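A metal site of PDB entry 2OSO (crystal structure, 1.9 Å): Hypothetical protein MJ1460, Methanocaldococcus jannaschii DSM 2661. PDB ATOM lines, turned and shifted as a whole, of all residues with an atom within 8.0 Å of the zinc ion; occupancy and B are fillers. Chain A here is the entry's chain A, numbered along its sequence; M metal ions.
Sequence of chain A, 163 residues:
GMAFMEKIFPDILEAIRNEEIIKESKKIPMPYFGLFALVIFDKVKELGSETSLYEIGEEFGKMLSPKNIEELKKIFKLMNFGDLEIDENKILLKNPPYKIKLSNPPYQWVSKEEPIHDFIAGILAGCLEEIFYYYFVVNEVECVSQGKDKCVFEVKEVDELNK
OE1 of Glu 140 lies within hydrogen-bond range of N of Ile 116 (3.5 Å).
O of Pro 106 lies within hydrogen-bond range of NE2 of His 117 (2.8 Å).
SG of Cys 151 lies close to N of Val 144.
The backbone carbonyl oxygen (O) of Cys 151 sits at hydrogen-bond distance from the backbone NH (N) of Leu 102.
The side-chain sulfur (SG) of Cys 143 sits close to the backbone NH (N) of Ile 116, at 3.5 Å.
The side-chain sulfur (SG) of Cys 143 lies close to the backbone NH (N) of Ser 145 (3.6 Å).
N of Cys 143 sits at hydrogen-bond distance from OE1 of Gln 146.
The nearest printed residue that does not touch the zinc ion is Val 144 (4.1 Å).
The zinc ion is bound by the side-chain carboxylate (OE2) of Glu 140 (1.9 Å), a ring nitrogen (ND1) of His 117 (2.1 Å), the side-chain sulfur (SG) of Cys 151 (2.3 Å) and the side-chain sulfur (SG) of Cys 143 (2.4 Å).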
ATOM      1  N   LEU A 102     -27.709 -12.423  10.082  1.00  0.00           N
ATOM      2  CA  LEU A 102     -26.470 -11.791  10.472  1.00  0.00           C
ATOM      3  C   LEU A 102     -26.441 -10.230  10.253  1.00  0.00           C
ATOM      4  O   LEU A 102     -26.759  -9.690   9.173  1.00  0.00           O
ATOM      5  CB  LEU A 102     -25.300 -12.516   9.811  1.00  0.00           C
ATOM      6  CG  LEU A 102     -23.873 -12.070  10.166  1.00  0.00           C
ATOM      7  CD1 LEU A 102     -23.417 -12.445  11.592  1.00  0.00           C
ATOM      8  CD2 LEU A 102     -22.947 -12.698   9.097  1.00  0.00           C
ATOM      9  N   PRO A 105     -21.984  -7.817   8.977  1.00  0.00           N
ATOM     10  CA  PRO A 105     -21.153  -8.877   8.422  1.00  0.00           C
ATOM     11  C   PRO A 105     -19.896  -8.276   7.739  1.00  0.00           C
ATOM     12  O   PRO A 105     -19.792  -7.061   7.645  1.00  0.00           O
ATOM     13  CB  PRO A 105     -22.050  -9.528   7.389  1.00  0.00           C
ATOM     14  CG  PRO A 105     -22.800  -8.298   6.828  1.00  0.00           C
ATOM     15  CD  PRO A 105     -23.069  -7.447   8.048  1.00  0.00           C
ATOM     16  N   PRO A 106     -18.937  -9.112   7.332  1.00  0.00           N
ATOM     17  CA  PRO A 106     -17.848  -8.559   6.521  1.00  0.00           C
ATOM     18  C   PRO A 106     -18.311  -8.210   5.108  1.00  0.00           C
ATOM     19  O   PRO A 106     -19.443  -8.525   4.702  1.00  0.00           O
ATOM     20  CB  PRO A 106     -16.797  -9.702   6.502  1.00  0.00           C
ATOM     21  CG  PRO A 106     -17.310 -10.755   7.332  1.00  0.00           C
ATOM     22  CD  PRO A 106     -18.723 -10.534   7.672  1.00  0.00           C
ATOM     23  N   TYR A 107     -17.423  -7.535   4.380  1.00  0.00           N
ATOM     24  CA  TYR A 107     -17.591  -7.235   2.967  1.00  0.00           C
ATOM     25  C   TYR A 107     -18.748  -6.295   2.680  1.00  0.00           C
ATOM     26  O   TYR A 107     -19.375  -6.460   1.667  1.00  0.00           O
ATOM     27  CB  TYR A 107     -17.815  -8.512   2.160  1.00  0.00           C
ATOM     28  CG  TYR A 107     -16.675  -9.468   2.238  1.00  0.00           C
ATOM     29  CD1 TYR A 107     -15.402  -9.068   1.857  1.00  0.00           C
ATOM     30  CD2 TYR A 107     -16.863 -10.780   2.633  1.00  0.00           C
ATOM     31  CE1 TYR A 107     -14.353  -9.922   1.898  1.00  0.00           C
ATOM     32  CE2 TYR A 107     -15.813 -11.665   2.672  1.00  0.00           C
ATOM     33  CZ  TYR A 107     -14.544 -11.224   2.294  1.00  0.00           C
ATOM     34  OH  TYR A 107     -13.421 -12.041   2.327  1.00  0.00           O
ATOM     35  N   GLU A 114     -26.392 -11.064  -6.089  1.00  0.00           N
ATOM     36  CA  GLU A 114     -26.573 -12.359  -5.514  1.00  0.00           C
ATOM     37  C   GLU A 114     -25.885 -12.327  -4.129  1.00  0.00           C
ATOM     38  O   GLU A 114     -24.924 -11.558  -3.927  1.00  0.00           O
ATOM     39  CB  GLU A 114     -25.957 -13.418  -6.413  1.00  0.00           C
ATOM     40  CG  GLU A 114     -26.727 -14.708  -6.487  1.00  0.00           C
ATOM     41  CD  GLU A 114     -26.991 -15.153  -7.918  1.00  0.00           C
ATOM     42  N   PRO A 115     -26.419 -13.096  -3.178  1.00  0.00           N
ATOM     43  CA  PRO A 115     -25.811 -13.182  -1.828  1.00  0.00           C
ATOM     44  C   PRO A 115     -24.365 -13.639  -1.885  1.00  0.00           C
ATOM     45  O   PRO A 115     -24.044 -14.509  -2.728  1.00  0.00           O
ATOM     46  CB  PRO A 115     -26.726 -14.205  -1.117  1.00  0.00           C
ATOM     47  CG  PRO A 115     -27.947 -14.152  -1.750  1.00  0.00           C
ATOM     48  CD  PRO A 115     -27.661 -13.900  -3.226  1.00  0.00           C
ATOM     49  N   ILE A 116     -23.494 -13.141  -0.962  1.00  0.00           N
ATOM     50  CA  ILE A 116     -22.034 -13.344  -1.105  1.00  0.00           C
ATOM     51  C   ILE A 116     -21.370 -14.193  -0.018  1.00  0.00           C
ATOM     52  O   ILE A 116     -20.249 -14.501  -0.169  1.00  0.00           O
ATOM     53  CB  ILE A 116     -21.213 -12.016  -1.300  1.00  0.00           C
ATOM     54  CG1 ILE A 116     -21.352 -11.031  -0.107  1.00  0.00           C
ATOM     55  CG2 ILE A 116     -21.720 -11.266  -2.645  1.00  0.00           C
ATOM     56  CD1 ILE A 116     -20.352  -9.920  -0.097  1.00  0.00           C
ATOM     57  N   HIS A 117     -22.073 -14.515   1.052  1.00  0.00           N
ATOM     58  CA  HIS A 117     -21.418 -14.960   2.268  1.00  0.00           C
ATOM     59  C   HIS A 117     -21.495 -16.498   2.302  1.00  0.00           C
ATOM     60  O   HIS A 117     -21.994 -17.086   3.265  1.00  0.00           O
ATOM     61  CB  HIS A 117     -22.047 -14.297   3.489  1.00  0.00           C
ATOM     62  CG  HIS A 117     -21.681 -12.860   3.650  1.00  0.00           C
ATOM     63  ND1 HIS A 117     -22.571 -11.830   3.377  1.00  0.00           N
ATOM     64  CD2 HIS A 117     -20.494 -12.266   3.899  1.00  0.00           C
ATOM     65  CE1 HIS A 117     -21.960 -10.670   3.586  1.00  0.00           C
ATOM     66  NE2 HIS A 117     -20.700 -10.905   3.898  1.00  0.00           N
ATOM     67  N   ASP A 118     -20.930 -17.115   1.259  1.00  0.00           N
ATOM     68  CA  ASP A 118     -20.876 -18.581   1.114  1.00  0.00           C
ATOM     69  C   ASP A 118     -20.032 -19.273   2.207  1.00  0.00           C
ATOM     70  O   ASP A 118     -20.420 -20.342   2.664  1.00  0.00           O
ATOM     71  CB  ASP A 118     -20.240 -19.013  -0.202  1.00  0.00           C
ATOM     72  CG  ASP A 118     -21.102 -18.771  -1.394  1.00  0.00           C
ATOM     73  OD1 ASP A 118     -22.107 -18.040  -1.304  1.00  0.00           O
ATOM     74  OD2 ASP A 118     -20.709 -19.307  -2.443  1.00  0.00           O
ATOM     75  N   ILE A 120     -19.408 -18.040   5.287  1.00  0.00           N
ATOM     76  CA  ILE A 120     -20.203 -17.940   6.530  1.00  0.00           C
ATOM     77  C   ILE A 120     -21.365 -18.975   6.564  1.00  0.00           C
ATOM     78  O   ILE A 120     -21.640 -19.634   7.587  1.00  0.00           O
ATOM     79  CB  ILE A 120     -20.743 -16.462   6.762  1.00  0.00           C
ATOM     80  CG1 ILE A 120     -19.615 -15.516   7.224  1.00  0.00           C
ATOM     81  CG2 ILE A 120     -21.967 -16.508   7.722  1.00  0.00           C
ATOM     82  CD1 ILE A 120     -19.979 -14.010   7.321  1.00  0.00           C
ATOM     83  N   GLU A 140     -28.088 -18.788   1.848  1.00  0.00           N
ATOM     84  CA  GLU A 140     -28.244 -17.380   2.140  1.00  0.00           C
ATOM     85  C   GLU A 140     -29.221 -16.889   1.085  1.00  0.00           C
ATOM     86  O   GLU A 140     -28.969 -17.046  -0.105  1.00  0.00           O
ATOM     87  CB  GLU A 140     -26.898 -16.602   2.104  1.00  0.00           C
ATOM     88  CG  GLU A 140     -27.047 -15.142   2.556  1.00  0.00           C
ATOM     89  CD  GLU A 140     -25.752 -14.373   2.529  1.00  0.00           C
ATOM     90  OE1 GLU A 140     -24.825 -14.799   1.818  1.00  0.00           O
ATOM     91  OE2 GLU A 140     -25.659 -13.310   3.190  1.00  0.00           O
ATOM     92  N   VAL A 141     -30.323 -16.303   1.545  1.00  0.00           N
ATOM     93  CA  VAL A 141     -31.404 -15.874   0.659  1.00  0.00           C
ATOM     94  C   VAL A 141     -31.522 -14.356   0.605  1.00  0.00           C
ATOM     95  O   VAL A 141     -32.144 -13.831  -0.300  1.00  0.00           O
ATOM     96  CB  VAL A 141     -32.751 -16.534   1.108  1.00  0.00           C
ATOM     97  CG1 VAL A 141     -32.661 -18.123   1.075  1.00  0.00           C
ATOM     98  CG2 VAL A 141     -33.153 -16.061   2.536  1.00  0.00           C
ATOM     99  N   GLU A 142     -30.993 -13.633   1.592  1.00  0.00           N
ATOM    100  CA  GLU A 142     -30.874 -12.155   1.486  1.00  0.00           C
ATOM    101  C   GLU A 142     -29.503 -11.735   2.025  1.00  0.00           C
ATOM    102  O   GLU A 142     -28.958 -12.383   2.926  1.00  0.00           O
ATOM    103  CB  GLU A 142     -31.960 -11.400   2.277  1.00  0.00           C
ATOM    104  CG  GLU A 142     -33.372 -11.861   2.120  1.00  0.00           C
ATOM    105  CD  GLU A 142     -34.375 -11.059   2.996  1.00  0.00           C
ATOM    106  OE1 GLU A 142     -34.022 -10.012   3.575  1.00  0.00           O
ATOM    107  OE2 GLU A 142     -35.519 -11.514   3.120  1.00  0.00           O
ATOM    108  N   CYS A 143     -28.974 -10.613   1.545  1.00  0.00           N
ATOM    109  CA  CYS A 143     -27.576 -10.245   1.921  1.00  0.00           C
ATOM    110  C   CYS A 143     -27.408  -8.715   1.937  1.00  0.00           C
ATOM    111  O   CYS A 143     -28.034  -8.017   1.144  1.00  0.00           O
ATOM    112  CB  CYS A 143     -26.629 -10.919   0.918  1.00  0.00           C
ATOM    113  SG  CYS A 143     -24.865 -10.655   1.126  1.00  0.00           S
ATOM    114  N   VAL A 144     -26.601  -8.220   2.873  1.00  0.00           N
ATOM    115  CA  VAL A 144     -26.268  -6.794   3.026  1.00  0.00           C
ATOM    116  C   VAL A 144     -25.708  -6.238   1.715  1.00  0.00           C
ATOM    117  O   VAL A 144     -25.965  -5.091   1.333  1.00  0.00           O
ATOM    118  CB  VAL A 144     -25.290  -6.602   4.233  1.00  0.00           C
ATOM    119  CG1 VAL A 144     -24.734  -5.151   4.308  1.00  0.00           C
ATOM    120  CG2 VAL A 144     -25.987  -6.987   5.515  1.00  0.00           C
ATOM    121  N   SER A 145     -24.991  -7.084   0.973  1.00  0.00           N
ATOM    122  CA  SER A 145     -24.375  -6.626  -0.265  1.00  0.00           C
ATOM    123  C   SER A 145     -25.389  -6.489  -1.398  1.00  0.00           C
ATOM    124  O   SER A 145     -25.080  -5.910  -2.447  1.00  0.00           O
ATOM    125  CB  SER A 145     -23.183  -7.531  -0.616  1.00  0.00           C
ATOM    126  OG  SER A 145     -22.129  -7.357   0.324  1.00  0.00           O
ATOM    127  N   GLN A 146     -26.616  -6.956  -1.177  1.00  0.00           N
ATOM    128  CA  GLN A 146     -27.760  -6.614  -2.050  1.00  0.00           C
ATOM    129  C   GLN A 146     -28.459  -5.298  -1.683  1.00  0.00           C
ATOM    130  O   GLN A 146     -29.410  -4.913  -2.341  1.00  0.00           O
ATOM    131  CB  GLN A 146     -28.836  -7.700  -2.051  1.00  0.00           C
ATOM    132  CG  GLN A 146     -28.344  -9.134  -2.392  1.00  0.00           C
ATOM    133  CD  GLN A 146     -29.475 -10.146  -2.165  1.00  0.00           C
ATOM    134  OE1 GLN A 146     -30.085 -10.167  -1.105  1.00  0.00           O
ATOM    135  NE2 GLN A 146     -29.764 -10.975  -3.175  1.00  0.00           N
ATOM    136  N   LYS A 148     -29.628  -4.916   1.534  1.00  0.00           N
ATOM    137  CA  LYS A 148     -30.424  -5.266   2.716  1.00  0.00           C
ATOM    138  C   LYS A 148     -29.705  -4.844   3.999  1.00  0.00           C
ATOM    139  O   LYS A 148     -28.489  -4.565   3.994  1.00  0.00           O
ATOM    140  CB  LYS A 148     -30.729  -6.759   2.713  1.00  0.00           C
ATOM    141  CG  LYS A 148     -31.551  -7.228   1.503  1.00  0.00           C
ATOM    142  CD  LYS A 148     -32.904  -6.591   1.428  1.00  0.00           C
ATOM    143  CE  LYS A 148     -34.032  -7.462   1.926  1.00  0.00           C
ATOM    144  NZ  LYS A 148     -35.316  -6.904   1.478  1.00  0.00           N
ATOM    145  N   LYS A 150     -29.605  -6.665   6.864  1.00  0.00           N
ATOM    146  CA  LYS A 150     -29.067  -7.835   7.532  1.00  0.00           C
ATOM    147  C   LYS A 150     -28.993  -8.918   6.482  1.00  0.00           C
ATOM    148  O   LYS A 150     -29.759  -8.892   5.517  1.00  0.00           O
ATOM    149  CB  LYS A 150     -30.019  -8.282   8.656  1.00  0.00           C
ATOM    150  CG  LYS A 150     -30.298  -7.231   9.734  1.00  0.00           C
ATOM    151  CD  LYS A 150     -31.041  -7.835  10.879  1.00  0.00           C
ATOM    152  CE  LYS A 150     -31.453  -6.821  11.901  1.00  0.00           C
ATOM    153  NZ  LYS A 150     -32.424  -7.483  12.782  1.00  0.00           N
ATOM    154  N   CYS A 151     -28.070  -9.864   6.635  1.00  0.00           N
ATOM    155  CA  CYS A 151     -28.086 -11.090   5.822  1.00  0.00           C
ATOM    156  C   CYS A 151     -29.049 -12.087   6.466  1.00  0.00           C
ATOM    157  O   CYS A 151     -29.159 -12.125   7.704  1.00  0.00           O
ATOM    158  CB  CYS A 151     -26.710 -11.707   5.683  1.00  0.00           C
ATOM    159  SG  CYS A 151     -25.323 -10.610   5.054  1.00  0.00           S
ATOM    160  N   VAL A 152     -29.701 -12.898   5.634  1.00  0.00           N
ATOM    161  CA  VAL A 152     -30.667 -13.895   6.065  1.00  0.00           C
ATOM    162  C   VAL A 152     -30.328 -15.256   5.463  1.00  0.00           C
ATOM    163  O   VAL A 152     -30.165 -15.408   4.255  1.00  0.00           O
ATOM    164  CB  VAL A 152     -32.087 -13.514   5.700  1.00  0.00           C
ATOM    165  CG1 VAL A 152     -33.065 -14.608   6.177  1.00  0.00           C
ATOM    166  CG2 VAL A 152     -32.457 -12.150   6.282  1.00  0.00           C
ATOM    167  N   PHE A 153     -30.252 -16.234   6.351  1.00  0.00           N
ATOM    168  CA  PHE A 153     -29.928 -17.619   6.013  1.00  0.00           C
ATOM    169  C   PHE A 153     -31.096 -18.553   6.343  1.00  0.00           C
ATOM    170  O   PHE A 153     -31.627 -18.536   7.469  1.00  0.00           O
ATOM    171  CB  PHE A 153     -28.686 -18.058   6.771  1.00  0.00           C
ATOM    172  CG  PHE A 153     -27.456 -17.165   6.556  1.00  0.00           C
ATOM    173  CD1 PHE A 153     -27.250 -16.021   7.357  1.00  0.00           C
ATOM    174  CD2 PHE A 153     -26.495 -17.478   5.608  1.00  0.00           C
ATOM    175  CE1 PHE A 153     -26.101 -15.217   7.195  1.00  0.00           C
ATOM    176  CE2 PHE A 153     -25.338 -16.644   5.411  1.00  0.00           C
ATOM    177  CZ  PHE A 153     -25.141 -15.540   6.236  1.00  0.00           C
HETATM  178 ZN    ZN M   1     -24.613 -11.745   3.201  1.00  0.00          ZN
